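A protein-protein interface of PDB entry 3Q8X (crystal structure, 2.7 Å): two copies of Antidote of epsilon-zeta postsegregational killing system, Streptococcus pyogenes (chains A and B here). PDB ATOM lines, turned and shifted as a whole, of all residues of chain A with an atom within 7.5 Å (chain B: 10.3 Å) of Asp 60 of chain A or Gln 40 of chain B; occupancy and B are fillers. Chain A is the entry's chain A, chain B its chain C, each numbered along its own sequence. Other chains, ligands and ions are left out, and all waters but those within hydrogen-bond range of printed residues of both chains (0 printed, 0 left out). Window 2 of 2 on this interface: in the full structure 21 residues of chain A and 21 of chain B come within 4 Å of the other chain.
The backbone carbonyl oxygen of Leu 52 of chain A is in hydrogen-bond range of the side-chain amide nitrogen of Asn 45 of chain B (3.1 Å).
The side-chain amide oxygen (OE1) of Gln 40 of chain B lies within hydrogen-bond range of the backbone NH (N) of Asn 57 of chain A (2.7 Å).
O of Gln 40 of chain B is in hydrogen-bond range of OH of Tyr 61 of chain A (2.6 Å).
The side-chain hydroxyl (OH) of Tyr 61 of chain A sits at hydrogen-bond distance from the backbone NH (N) of Leu 42 of chain B (3.4 Å).
No position is printed for both chains.
Hydrophobic or aromatic side chains of chain A that line the printed part of chain B: Leu 52, Val 56 and Tyr 61.
Of the 16 printed residues of chain B, 7 touch a printed residue of chain A.
Among the printed residues, 12 pairs touch across the chains.
Among the printed residues, no Asp or Glu carboxylate lies within 4 Å of a Lys or Arg side-chain nitrogen of the other chain.
Asp 60 of chain A touches one residue of chain B.
Gln 40 of chain B touches just these residues of chain A: Val 56 (3.4 Å), Asn 57 (2.7 Å), Asp 60 (3.7 Å) and Tyr 61 (2.6 Å).
Of the printed residues of chain B, Val 56 of chain A touches Ser 39 (3.8 Å), Gln 40 (3.4 Å) and Asn 45 (3.8 Å).
Asn 57 of chain A touches just one residue of chain B: Gln 40 (2.7 Å).
Of chain B, only Gln 40 (2.6 Å), Leu 41 (3.96 Å) and Leu 42 (3.4 Å) come within 4 Å of Tyr 61 of chain A.
Printed residues of chain B within 4 Å of Glu 65 of chain A: Leu 42 (3.5 Å).
Of the printed residues of chain A, Leu 41 of chain B touches Tyr 61.
Asp 38 of chain B touches none of the printed residues of chain A.
O of Tyr 61 of chain A sits at hydrogen-bond distance from NZ of Lys 7 of chain A.
N of Ser 62 of chain A sits at hydrogen-bond distance from OE1 of Glu 65 of chain A (3.2 Å).
The backbone NH (N) of Gln 40 of chain B lies close to the side-chain carboxylate (OD1) of Asp 38 of chain B, at 3.3 Å.
The backbone carbonyl oxygen of Ser 39 of chain B is in hydrogen-bond range of the side-chain amide nitrogen of Asn 45 of chain B (3.1 Å).
ND2 of Asn 48 of chain B sits at hydrogen-bond distance from O of Val 44 of chain B (3.3 Å).
The side-chain amide oxygen (OD1) of Asn 45 of chain B is in hydrogen-bond range of the side-chain amide nitrogen (NE2) of Gln 49 of chain B (2.9 Å).
Among the printed residues, pairs that only touch across the chains: Leu 52 of chain A with Asn 48 of chain B, Leu 52 of chain A with Gln 49 of chain B, Val 56 of chain A with Ser 39 of chain B, Val 56 of chain A with Gln 40 of chain B, Val 56 of chain A with Asn 45 of chain B, Asp 60 of chain A with Gln 40 of chain B, Tyr 61 of chain A with Leu 41 of chain B and Glu 65 of chain A with Leu 42 of chain B.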
ATOM      1  N   LYS A   7       8.355  -5.194   2.311  1.00  0.00           N
ATOM      2  CA  LYS A   7       7.472  -4.942   1.176  1.00  0.00           C
ATOM      3  C   LYS A   7       7.036  -3.488   1.149  1.00  0.00           C
ATOM      4  O   LYS A   7       7.120  -2.854   0.105  1.00  0.00           O
ATOM      5  CB  LYS A   7       6.265  -5.890   1.162  1.00  0.00           C
ATOM      6  CG  LYS A   7       6.644  -7.347   0.892  1.00  0.00           C
ATOM      7  CD  LYS A   7       5.513  -8.140   0.249  1.00  0.00           C
ATOM      8  CE  LYS A   7       4.501  -8.650   1.281  1.00  0.00           C
ATOM      9  NZ  LYS A   7       3.468  -9.513   0.625  1.00  0.00           N
ATOM     10  N   ILE A  11       7.687  -0.886  -1.950  1.00  0.00           N
ATOM     11  CA  ILE A  11       6.595  -0.157  -2.568  1.00  0.00           C
ATOM     12  C   ILE A  11       6.849   1.361  -2.534  1.00  0.00           C
ATOM     13  O   ILE A  11       6.585   2.044  -3.518  1.00  0.00           O
ATOM     14  CB  ILE A  11       5.223  -0.554  -1.978  1.00  0.00           C
ATOM     15  CG1 ILE A  11       4.942  -2.044  -2.257  1.00  0.00           C
ATOM     16  CG2 ILE A  11       4.111   0.323  -2.549  1.00  0.00           C
ATOM     17  CD1 ILE A  11       3.833  -2.661  -1.397  1.00  0.00           C
ATOM     18  N   LEU A  52      -0.284   1.197 -18.386  1.00  0.00           N
ATOM     19  CA  LEU A  52      -0.632  -0.167 -17.986  1.00  0.00           C
ATOM     20  C   LEU A  52       0.132  -0.603 -16.736  1.00  0.00           C
ATOM     21  O   LEU A  52      -0.441  -1.198 -15.831  1.00  0.00           O
ATOM     22  CB  LEU A  52      -0.355  -1.166 -19.110  1.00  0.00           C
ATOM     23  CG  LEU A  52      -1.151  -1.116 -20.411  1.00  0.00           C
ATOM     24  CD1 LEU A  52      -0.608  -2.155 -21.389  1.00  0.00           C
ATOM     25  CD2 LEU A  52      -2.644  -1.333 -20.172  1.00  0.00           C
ATOM     26  N   ARG A  55      -1.241   0.553 -13.407  1.00  0.00           N
ATOM     27  CA  ARG A  55      -2.606   0.204 -13.033  1.00  0.00           C
ATOM     28  C   ARG A  55      -2.697  -0.820 -11.911  1.00  0.00           C
ATOM     29  O   ARG A  55      -3.767  -1.006 -11.315  1.00  0.00           O
ATOM     30  CB  ARG A  55      -3.383  -0.275 -14.239  1.00  0.00           C
ATOM     31  CG  ARG A  55      -3.960   0.858 -14.996  1.00  0.00           C
ATOM     32  CD  ARG A  55      -4.692   0.357 -16.197  1.00  0.00           C
ATOM     33  NE  ARG A  55      -4.698   1.395 -17.214  1.00  0.00           N
ATOM     34  CZ  ARG A  55      -5.184   1.239 -18.441  1.00  0.00           C
ATOM     35  NH1 ARG A  55      -5.717   0.071 -18.812  1.00  0.00           N
ATOM     36  NH2 ARG A  55      -5.136   2.263 -19.292  1.00  0.00           N
ATOM     37  N   VAL A  56      -1.573  -1.468 -11.617  1.00  0.00           N
ATOM     38  CA  VAL A  56      -1.573  -2.618 -10.727  1.00  0.00           C
ATOM     39  C   VAL A  56      -1.678  -2.214  -9.263  1.00  0.00           C
ATOM     40  O   VAL A  56      -1.205  -1.154  -8.873  1.00  0.00           O
ATOM     41  CB  VAL A  56      -0.314  -3.502 -10.943  1.00  0.00           C
ATOM     42  CG1 VAL A  56      -0.227  -3.984 -12.403  1.00  0.00           C
ATOM     43  CG2 VAL A  56       0.923  -2.746 -10.573  1.00  0.00           C
ATOM     44  N   ASN A  57      -2.301  -3.062  -8.459  1.00  0.00           N
ATOM     45  CA  ASN A  57      -2.258  -2.895  -7.028  1.00  0.00           C
ATOM     46  C   ASN A  57      -1.018  -3.565  -6.463  1.00  0.00           C
ATOM     47  O   ASN A  57      -0.982  -4.789  -6.305  1.00  0.00           O
ATOM     48  CB  ASN A  57      -3.509  -3.479  -6.365  1.00  0.00           C
ATOM     49  CG  ASN A  57      -3.395  -3.521  -4.844  1.00  0.00           C
ATOM     50  OD1 ASN A  57      -2.567  -2.827  -4.256  1.00  0.00           O
ATOM     51  ND2 ASN A  57      -4.224  -4.342  -4.204  1.00  0.00           N
ATOM     52  N   LEU A  58      -0.019  -2.758  -6.124  1.00  0.00           N
ATOM     53  CA  LEU A  58       1.233  -3.280  -5.566  1.00  0.00           C
ATOM     54  C   LEU A  58       1.086  -3.954  -4.201  1.00  0.00           C
ATOM     55  O   LEU A  58       1.949  -4.731  -3.793  1.00  0.00           O
ATOM     56  CB  LEU A  58       2.296  -2.185  -5.519  1.00  0.00           C
ATOM     57  CG  LEU A  58       2.727  -1.600  -6.877  1.00  0.00           C
ATOM     58  CD1 LEU A  58       3.547  -0.327  -6.657  1.00  0.00           C
ATOM     59  CD2 LEU A  58       3.506  -2.619  -7.739  1.00  0.00           C
ATOM     60  N   PHE A  59      -0.010  -3.683  -3.499  1.00  0.00           N
ATOM     61  CA  PHE A  59      -0.195  -4.266  -2.166  1.00  0.00           C
ATOM     62  C   PHE A  59      -0.547  -5.742  -2.247  1.00  0.00           C
ATOM     63  O   PHE A  59      -0.470  -6.460  -1.260  1.00  0.00           O
ATOM     64  CB  PHE A  59      -1.226  -3.487  -1.330  1.00  0.00           C
ATOM     65  CG  PHE A  59      -0.866  -2.048  -1.127  1.00  0.00           C
ATOM     66  CD1 PHE A  59       0.258  -1.699  -0.384  1.00  0.00           C
ATOM     67  CD2 PHE A  59      -1.638  -1.038  -1.696  1.00  0.00           C
ATOM     68  CE1 PHE A  59       0.609  -0.359  -0.212  1.00  0.00           C
ATOM     69  CE2 PHE A  59      -1.298   0.303  -1.536  1.00  0.00           C
ATOM     70  CZ  PHE A  59      -0.173   0.645  -0.797  1.00  0.00           C
ATOM     71  N   ASP A  60      -0.913  -6.196  -3.434  1.00  0.00           N
ATOM     72  CA  ASP A  60      -1.244  -7.600  -3.622  1.00  0.00           C
ATOM     73  C   ASP A  60      -0.033  -8.448  -4.049  1.00  0.00           C
ATOM     74  O   ASP A  60      -0.144  -9.658  -4.206  1.00  0.00           O
ATOM     75  CB  ASP A  60      -2.383  -7.739  -4.627  1.00  0.00           C
ATOM     76  CG  ASP A  60      -3.311  -8.856  -4.271  1.00  0.00           C
ATOM     77  OD1 ASP A  60      -4.072  -8.680  -3.297  1.00  0.00           O
ATOM     78  OD2 ASP A  60      -3.277  -9.911  -4.950  1.00  0.00           O
ATOM     79  N   TYR A  61       1.120  -7.814  -4.217  1.00  0.00           N
ATOM     80  CA  TYR A  61       2.302  -8.521  -4.670  1.00  0.00           C
ATOM     81  C   TYR A  61       3.183  -9.061  -3.550  1.00  0.00           C
ATOM     82  O   TYR A  61       3.253  -8.498  -2.455  1.00  0.00           O
ATOM     83  CB  TYR A  61       3.140  -7.633  -5.591  1.00  0.00           C
ATOM     84  CG  TYR A  61       2.624  -7.502  -7.008  1.00  0.00           C
ATOM     85  CD1 TYR A  61       1.692  -8.392  -7.532  1.00  0.00           C
ATOM     86  CD2 TYR A  61       3.096  -6.499  -7.832  1.00  0.00           C
ATOM     87  CE1 TYR A  61       1.235  -8.264  -8.828  1.00  0.00           C
ATOM     88  CE2 TYR A  61       2.658  -6.373  -9.125  1.00  0.00           C
ATOM     89  CZ  TYR A  61       1.732  -7.252  -9.622  1.00  0.00           C
ATOM     90  OH  TYR A  61       1.315  -7.095 -10.924  1.00  0.00           O
ATOM     91  N   SER A  62       3.861 -10.163  -3.851  1.00  0.00           N
ATOM     92  CA  SER A  62       4.912 -10.689  -2.999  1.00  0.00           C
ATOM     93  C   SER A  62       6.213  -9.918  -3.224  1.00  0.00           C
ATOM     94  O   SER A  62       6.326  -9.110  -4.160  1.00  0.00           O
ATOM     95  CB  SER A  62       5.133 -12.178  -3.268  1.00  0.00           C
ATOM     96  OG  SER A  62       5.721 -12.376  -4.544  1.00  0.00           O
ATOM     97  N   GLU A  65       7.734 -10.593  -6.627  1.00  0.00           N
ATOM     98  CA  GLU A  65       6.986  -9.829  -7.608  1.00  0.00           C
ATOM     99  C   GLU A  65       7.339  -8.354  -7.502  1.00  0.00           C
ATOM    100  O   GLU A  65       7.556  -7.698  -8.520  1.00  0.00           O
ATOM    101  CB  GLU A  65       5.486 -10.056  -7.451  1.00  0.00           C
ATOM    102  CG  GLU A  65       5.050 -11.427  -7.924  1.00  0.00           C
ATOM    103  CD  GLU A  65       3.569 -11.690  -7.714  1.00  0.00           C
ATOM    104  OE1 GLU A  65       3.118 -11.758  -6.540  1.00  0.00           O
ATOM    105  OE2 GLU A  65       2.859 -11.839  -8.735  1.00  0.00           O
ATOM    106  N   LEU A  66       7.431  -7.836  -6.278  1.00  0.00           N
ATOM    107  CA  LEU A  66       7.794  -6.427  -6.081  1.00  0.00           C
ATOM    108  C   LEU A  66       9.188  -6.128  -6.618  1.00  0.00           C
ATOM    109  O   LEU A  66       9.406  -5.102  -7.268  1.00  0.00           O
ATOM    110  CB  LEU A  66       7.697  -6.022  -4.612  1.00  0.00           C
ATOM    111  CG  LEU A  66       6.272  -5.833  -4.088  1.00  0.00           C
ATOM    112  CD1 LEU A  66       6.292  -5.655  -2.590  1.00  0.00           C
ATOM    113  CD2 LEU A  66       5.557  -4.668  -4.766  1.00  0.00           C
ATOM    114  N   LEU B  34      -2.751 -18.584 -16.798  1.00  0.00           N
ATOM    115  CA  LEU B  34      -3.139 -17.300 -16.214  1.00  0.00           C
ATOM    116  C   LEU B  34      -4.245 -16.636 -17.023  1.00  0.00           C
ATOM    117  O   LEU B  34      -4.228 -16.660 -18.256  1.00  0.00           O
ATOM    118  CB  LEU B  34      -1.940 -16.355 -16.075  1.00  0.00           C
ATOM    119  CG  LEU B  34      -0.730 -16.805 -15.256  1.00  0.00           C
ATOM    120  CD1 LEU B  34       0.299 -15.692 -15.192  1.00  0.00           C
ATOM    121  CD2 LEU B  34      -1.127 -17.246 -13.861  1.00  0.00           C
ATOM    122  N   ASN B  35      -5.204 -16.047 -16.314  1.00  0.00           N
ATOM    123  CA  ASN B  35      -6.281 -15.294 -16.934  1.00  0.00           C
ATOM    124  C   ASN B  35      -5.717 -14.080 -17.683  1.00  0.00           C
ATOM    125  O   ASN B  35      -5.400 -13.041 -17.077  1.00  0.00           O
ATOM    126  CB  ASN B  35      -7.309 -14.877 -15.871  1.00  0.00           C
ATOM    127  CG  ASN B  35      -8.518 -14.165 -16.460  1.00  0.00           C
ATOM    128  OD1 ASN B  35      -8.675 -14.075 -17.677  1.00  0.00           O
ATOM    129  ND2 ASN B  35      -9.382 -13.658 -15.594  1.00  0.00           N
ATOM    130  N   LYS B  36      -5.590 -14.231 -19.002  1.00  0.00           N
ATOM    131  CA  LYS B  36      -5.091 -13.176 -19.895  1.00  0.00           C
ATOM    132  C   LYS B  36      -5.840 -11.840 -19.750  1.00  0.00           C
ATOM    133  O   LYS B  36      -5.350 -10.798 -20.185  1.00  0.00           O
ATOM    134  CB  LYS B  36      -5.177 -13.638 -21.354  1.00  0.00           C
ATOM    135  CG  LYS B  36      -4.573 -15.014 -21.652  1.00  0.00           C
ATOM    136  CD  LYS B  36      -5.104 -15.602 -22.978  1.00  0.00           C
ATOM    137  CE  LYS B  36      -4.204 -15.265 -24.184  1.00  0.00           C
ATOM    138  NZ  LYS B  36      -4.008 -13.802 -24.384  1.00  0.00           N
ATOM    139  N   ASN B  37      -7.029 -11.892 -19.153  1.00  0.00           N
ATOM    140  CA  ASN B  37      -7.868 -10.707 -18.925  1.00  0.00           C
ATOM    141  C   ASN B  37      -7.562  -9.965 -17.607  1.00  0.00           C
ATOM    142  O   ASN B  37      -8.097  -8.880 -17.351  1.00  0.00           O
ATOM    143  CB  ASN B  37      -9.359 -11.093 -18.979  1.00  0.00           C
ATOM    144  CG  ASN B  37      -9.798 -11.591 -20.359  1.00  0.00           C
ATOM    145  OD1 ASN B  37      -9.263 -11.169 -21.395  1.00  0.00           O
ATOM    146  ND2 ASN B  37     -10.782 -12.488 -20.376  1.00  0.00           N
ATOM    147  N   ASP B  38      -6.714 -10.569 -16.777  1.00  0.00           N
ATOM    148  CA  ASP B  38      -6.348 -10.009 -15.485  1.00  0.00           C
ATOM    149  C   ASP B  38      -4.991  -9.325 -15.602  1.00  0.00           C
ATOM    150  O   ASP B  38      -3.944  -9.922 -15.357  1.00  0.00           O
ATOM    151  CB  ASP B  38      -6.319 -11.109 -14.420  1.00  0.00           C
ATOM    152  CG  ASP B  38      -6.247 -10.561 -13.008  1.00  0.00           C
ATOM    153  OD1 ASP B  38      -6.213  -9.322 -12.835  1.00  0.00           O
ATOM    154  OD2 ASP B  38      -6.234 -11.380 -12.063  1.00  0.00           O
ATOM    155  N   SER B  39      -5.022  -8.061 -15.987  1.00  0.00           N
ATOM    156  CA  SER B  39      -3.806  -7.288 -16.155  1.00  0.00           C
ATOM    157  C   SER B  39      -3.122  -6.956 -14.808  1.00  0.00           C
ATOM    158  O   SER B  39      -2.085  -6.301 -14.778  1.00  0.00           O
ATOM    159  CB  SER B  39      -4.113  -6.025 -16.974  1.00  0.00           C
ATOM    160  OG  SER B  39      -5.215  -5.303 -16.420  1.00  0.00           O
ATOM    161  N   GLN B  40      -3.705  -7.419 -13.706  1.00  0.00           N
ATOM    162  CA  GLN B  40      -3.108  -7.263 -12.379  1.00  0.00           C
ATOM    163  C   GLN B  40      -1.956  -8.253 -12.182  1.00  0.00           C
ATOM    164  O   GLN B  40      -1.026  -7.992 -11.422  1.00  0.00           O
ATOM    165  CB  GLN B  40      -4.182  -7.411 -11.289  1.00  0.00           C
ATOM    166  CG  GLN B  40      -3.691  -7.634  -9.842  1.00  0.00           C
ATOM    167  CD  GLN B  40      -3.102  -6.389  -9.187  1.00  0.00           C
ATOM    168  OE1 GLN B  40      -3.354  -5.264  -9.611  1.00  0.00           O
ATOM    169  NE2 GLN B  40      -2.314  -6.593  -8.144  1.00  0.00           N
ATOM    170  N   LEU B  41      -2.017  -9.383 -12.878  1.00  0.00           N
ATOM    171  CA  LEU B  41      -0.956 -10.381 -12.825  1.00  0.00           C
ATOM    172  C   LEU B  41       0.282  -9.866 -13.557  1.00  0.00           C
ATOM    173  O   LEU B  41       0.204  -9.445 -14.716  1.00  0.00           O
ATOM    174  CB  LEU B  41      -1.428 -11.709 -13.425  1.00  0.00           C
ATOM    175  CG  LEU B  41      -2.724 -12.342 -12.882  1.00  0.00           C
ATOM    176  CD1 LEU B  41      -3.138 -13.525 -13.749  1.00  0.00           C
ATOM    177  CD2 LEU B  41      -2.638 -12.745 -11.403  1.00  0.00           C
ATOM    178  N   LEU B  42       1.418  -9.888 -12.866  1.00  0.00           N
ATOM    179  CA  LEU B  42       2.675  -9.369 -13.406  1.00  0.00           C
ATOM    180  C   LEU B  42       3.022  -9.885 -14.810  1.00  0.00           C
ATOM    181  O   LEU B  42       3.424  -9.112 -15.683  1.00  0.00           O
ATOM    182  CB  LEU B  42       3.808  -9.648 -12.419  1.00  0.00           C
ATOM    183  CG  LEU B  42       5.205  -9.054 -12.627  1.00  0.00           C
ATOM    184  CD1 LEU B  42       5.174  -7.615 -13.160  1.00  0.00           C
ATOM    185  CD2 LEU B  42       5.989  -9.122 -11.321  1.00  0.00           C
ATOM    186  N   GLU B  43       2.854 -11.182 -15.032  1.00  0.00           N
ATOM    187  CA  GLU B  43       3.227 -11.793 -16.312  1.00  0.00           C
ATOM    188  C   GLU B  43       2.231 -11.453 -17.418  1.00  0.00           C
ATOM    189  O   GLU B  43       2.590 -11.353 -18.581  1.00  0.00           O
ATOM    190  CB  GLU B  43       3.395 -13.309 -16.176  1.00  0.00           C
ATOM    191  CG  GLU B  43       4.400 -13.755 -15.100  1.00  0.00           C
ATOM    192  CD  GLU B  43       3.820 -13.808 -13.672  1.00  0.00           C
ATOM    193  OE1 GLU B  43       2.572 -13.838 -13.508  1.00  0.00           O
ATOM    194  OE2 GLU B  43       4.625 -13.825 -12.705  1.00  0.00           O
ATOM    195  N   VAL B  44       0.978 -11.260 -17.040  1.00  0.00           N
ATOM    196  CA  VAL B  44      -0.058 -10.861 -17.978  1.00  0.00           C
ATOM    197  C   VAL B  44       0.031  -9.353 -18.282  1.00  0.00           C
ATOM    198  O   VAL B  44      -0.280  -8.920 -19.389  1.00  0.00           O
ATOM    199  CB  VAL B  44      -1.468 -11.274 -17.457  1.00  0.00           C
ATOM    200  CG1 VAL B  44      -2.564 -10.801 -18.381  1.00  0.00           C
ATOM    201  CG2 VAL B  44      -1.556 -12.779 -17.313  1.00  0.00           C
ATOM    202  N   ASN B  45       0.466  -8.559 -17.308  1.00  0.00           N
ATOM    203  CA  ASN B  45       0.696  -7.136 -17.545  1.00  0.00           C
ATOM    204  C   ASN B  45       1.871  -6.912 -18.514  1.00  0.00           C
ATOM    205  O   ASN B  45       1.826  -6.029 -19.379  1.00  0.00           O
ATOM    206  CB  ASN B  45       0.927  -6.407 -16.230  1.00  0.00           C
ATOM    207  CG  ASN B  45       0.932  -4.893 -16.390  1.00  0.00           C
ATOM    208  OD1 ASN B  45       1.971  -4.290 -16.633  1.00  0.00           O
ATOM    209  ND2 ASN B  45      -0.228  -4.273 -16.225  1.00  0.00           N
ATOM    210  N   LEU B  46       2.912  -7.730 -18.375  1.00  0.00           N
ATOM    211  CA  LEU B  46       4.011  -7.710 -19.313  1.00  0.00           C
ATOM    212  C   LEU B  46       3.512  -8.012 -20.714  1.00  0.00           C
ATOM    213  O   LEU B  46       3.693  -7.205 -21.610  1.00  0.00           O
ATOM    214  CB  LEU B  46       5.083  -8.716 -18.904  1.00  0.00           C
ATOM    215  CG  LEU B  46       6.432  -8.649 -19.622  1.00  0.00           C
ATOM    216  CD1 LEU B  46       6.929  -7.222 -19.764  1.00  0.00           C
ATOM    217  CD2 LEU B  46       7.436  -9.484 -18.855  1.00  0.00           C
ATOM    218  N   LEU B  47       2.870  -9.164 -20.897  1.00  0.00           N
ATOM    219  CA  LEU B  47       2.329  -9.551 -22.197  1.00  0.00           C
ATOM    220  C   LEU B  47       1.582  -8.397 -22.854  1.00  0.00           C
ATOM    221  O   LEU B  47       1.828  -8.066 -24.018  1.00  0.00           O
ATOM    222  CB  LEU B  47       1.401 -10.753 -22.062  1.00  0.00           C
ATOM    223  CG  LEU B  47       0.986 -11.486 -23.343  1.00  0.00           C
ATOM    224  CD1 LEU B  47       2.161 -12.227 -23.947  1.00  0.00           C
ATOM    225  CD2 LEU B  47      -0.170 -12.450 -23.079  1.00  0.00           C
ATOM    226  N   ASN B  48       0.691  -7.765 -22.100  1.00  0.00           N
ATOM    227  CA  ASN B  48      -0.124  -6.690 -22.652  1.00  0.00           C
ATOM    228  C   ASN B  48       0.685  -5.494 -23.152  1.00  0.00           C
ATOM    229  O   ASN B  48       0.340  -4.881 -24.171  1.00  0.00           O
ATOM    230  CB  ASN B  48      -1.181  -6.262 -21.648  1.00  0.00           C
ATOM    231  CG  ASN B  48      -2.271  -7.279 -21.514  1.00  0.00           C
ATOM    232  OD1 ASN B  48      -2.525  -8.041 -22.441  1.00  0.00           O
ATOM    233  ND2 ASN B  48      -2.928  -7.303 -20.363  1.00  0.00           N
ATOM    234  N   GLN B  49       1.764  -5.176 -22.442  1.00  0.00           N
ATOM    235  CA  GLN B  49       2.674  -4.126 -22.874  1.00  0.00           C
ATOM    236  C   GLN B  49       3.328  -4.508 -24.186  1.00  0.00           C
ATOM    237  O   GLN B  49       3.419  -3.690 -25.093  1.00  0.00           O
ATOM    238  CB  GLN B  49       3.734  -3.878 -21.818  1.00  0.00           C
ATOM    239  CG  GLN B  49       3.172  -3.249 -20.586  1.00  0.00           C
ATOM    240  CD  GLN B  49       4.200  -3.075 -19.535  1.00  0.00           C
ATOM    241  OE1 GLN B  49       5.014  -2.159 -19.596  1.00  0.00           O
ATOM    242  NE2 GLN B  49       4.183  -3.955 -18.554  1.00  0.00           N
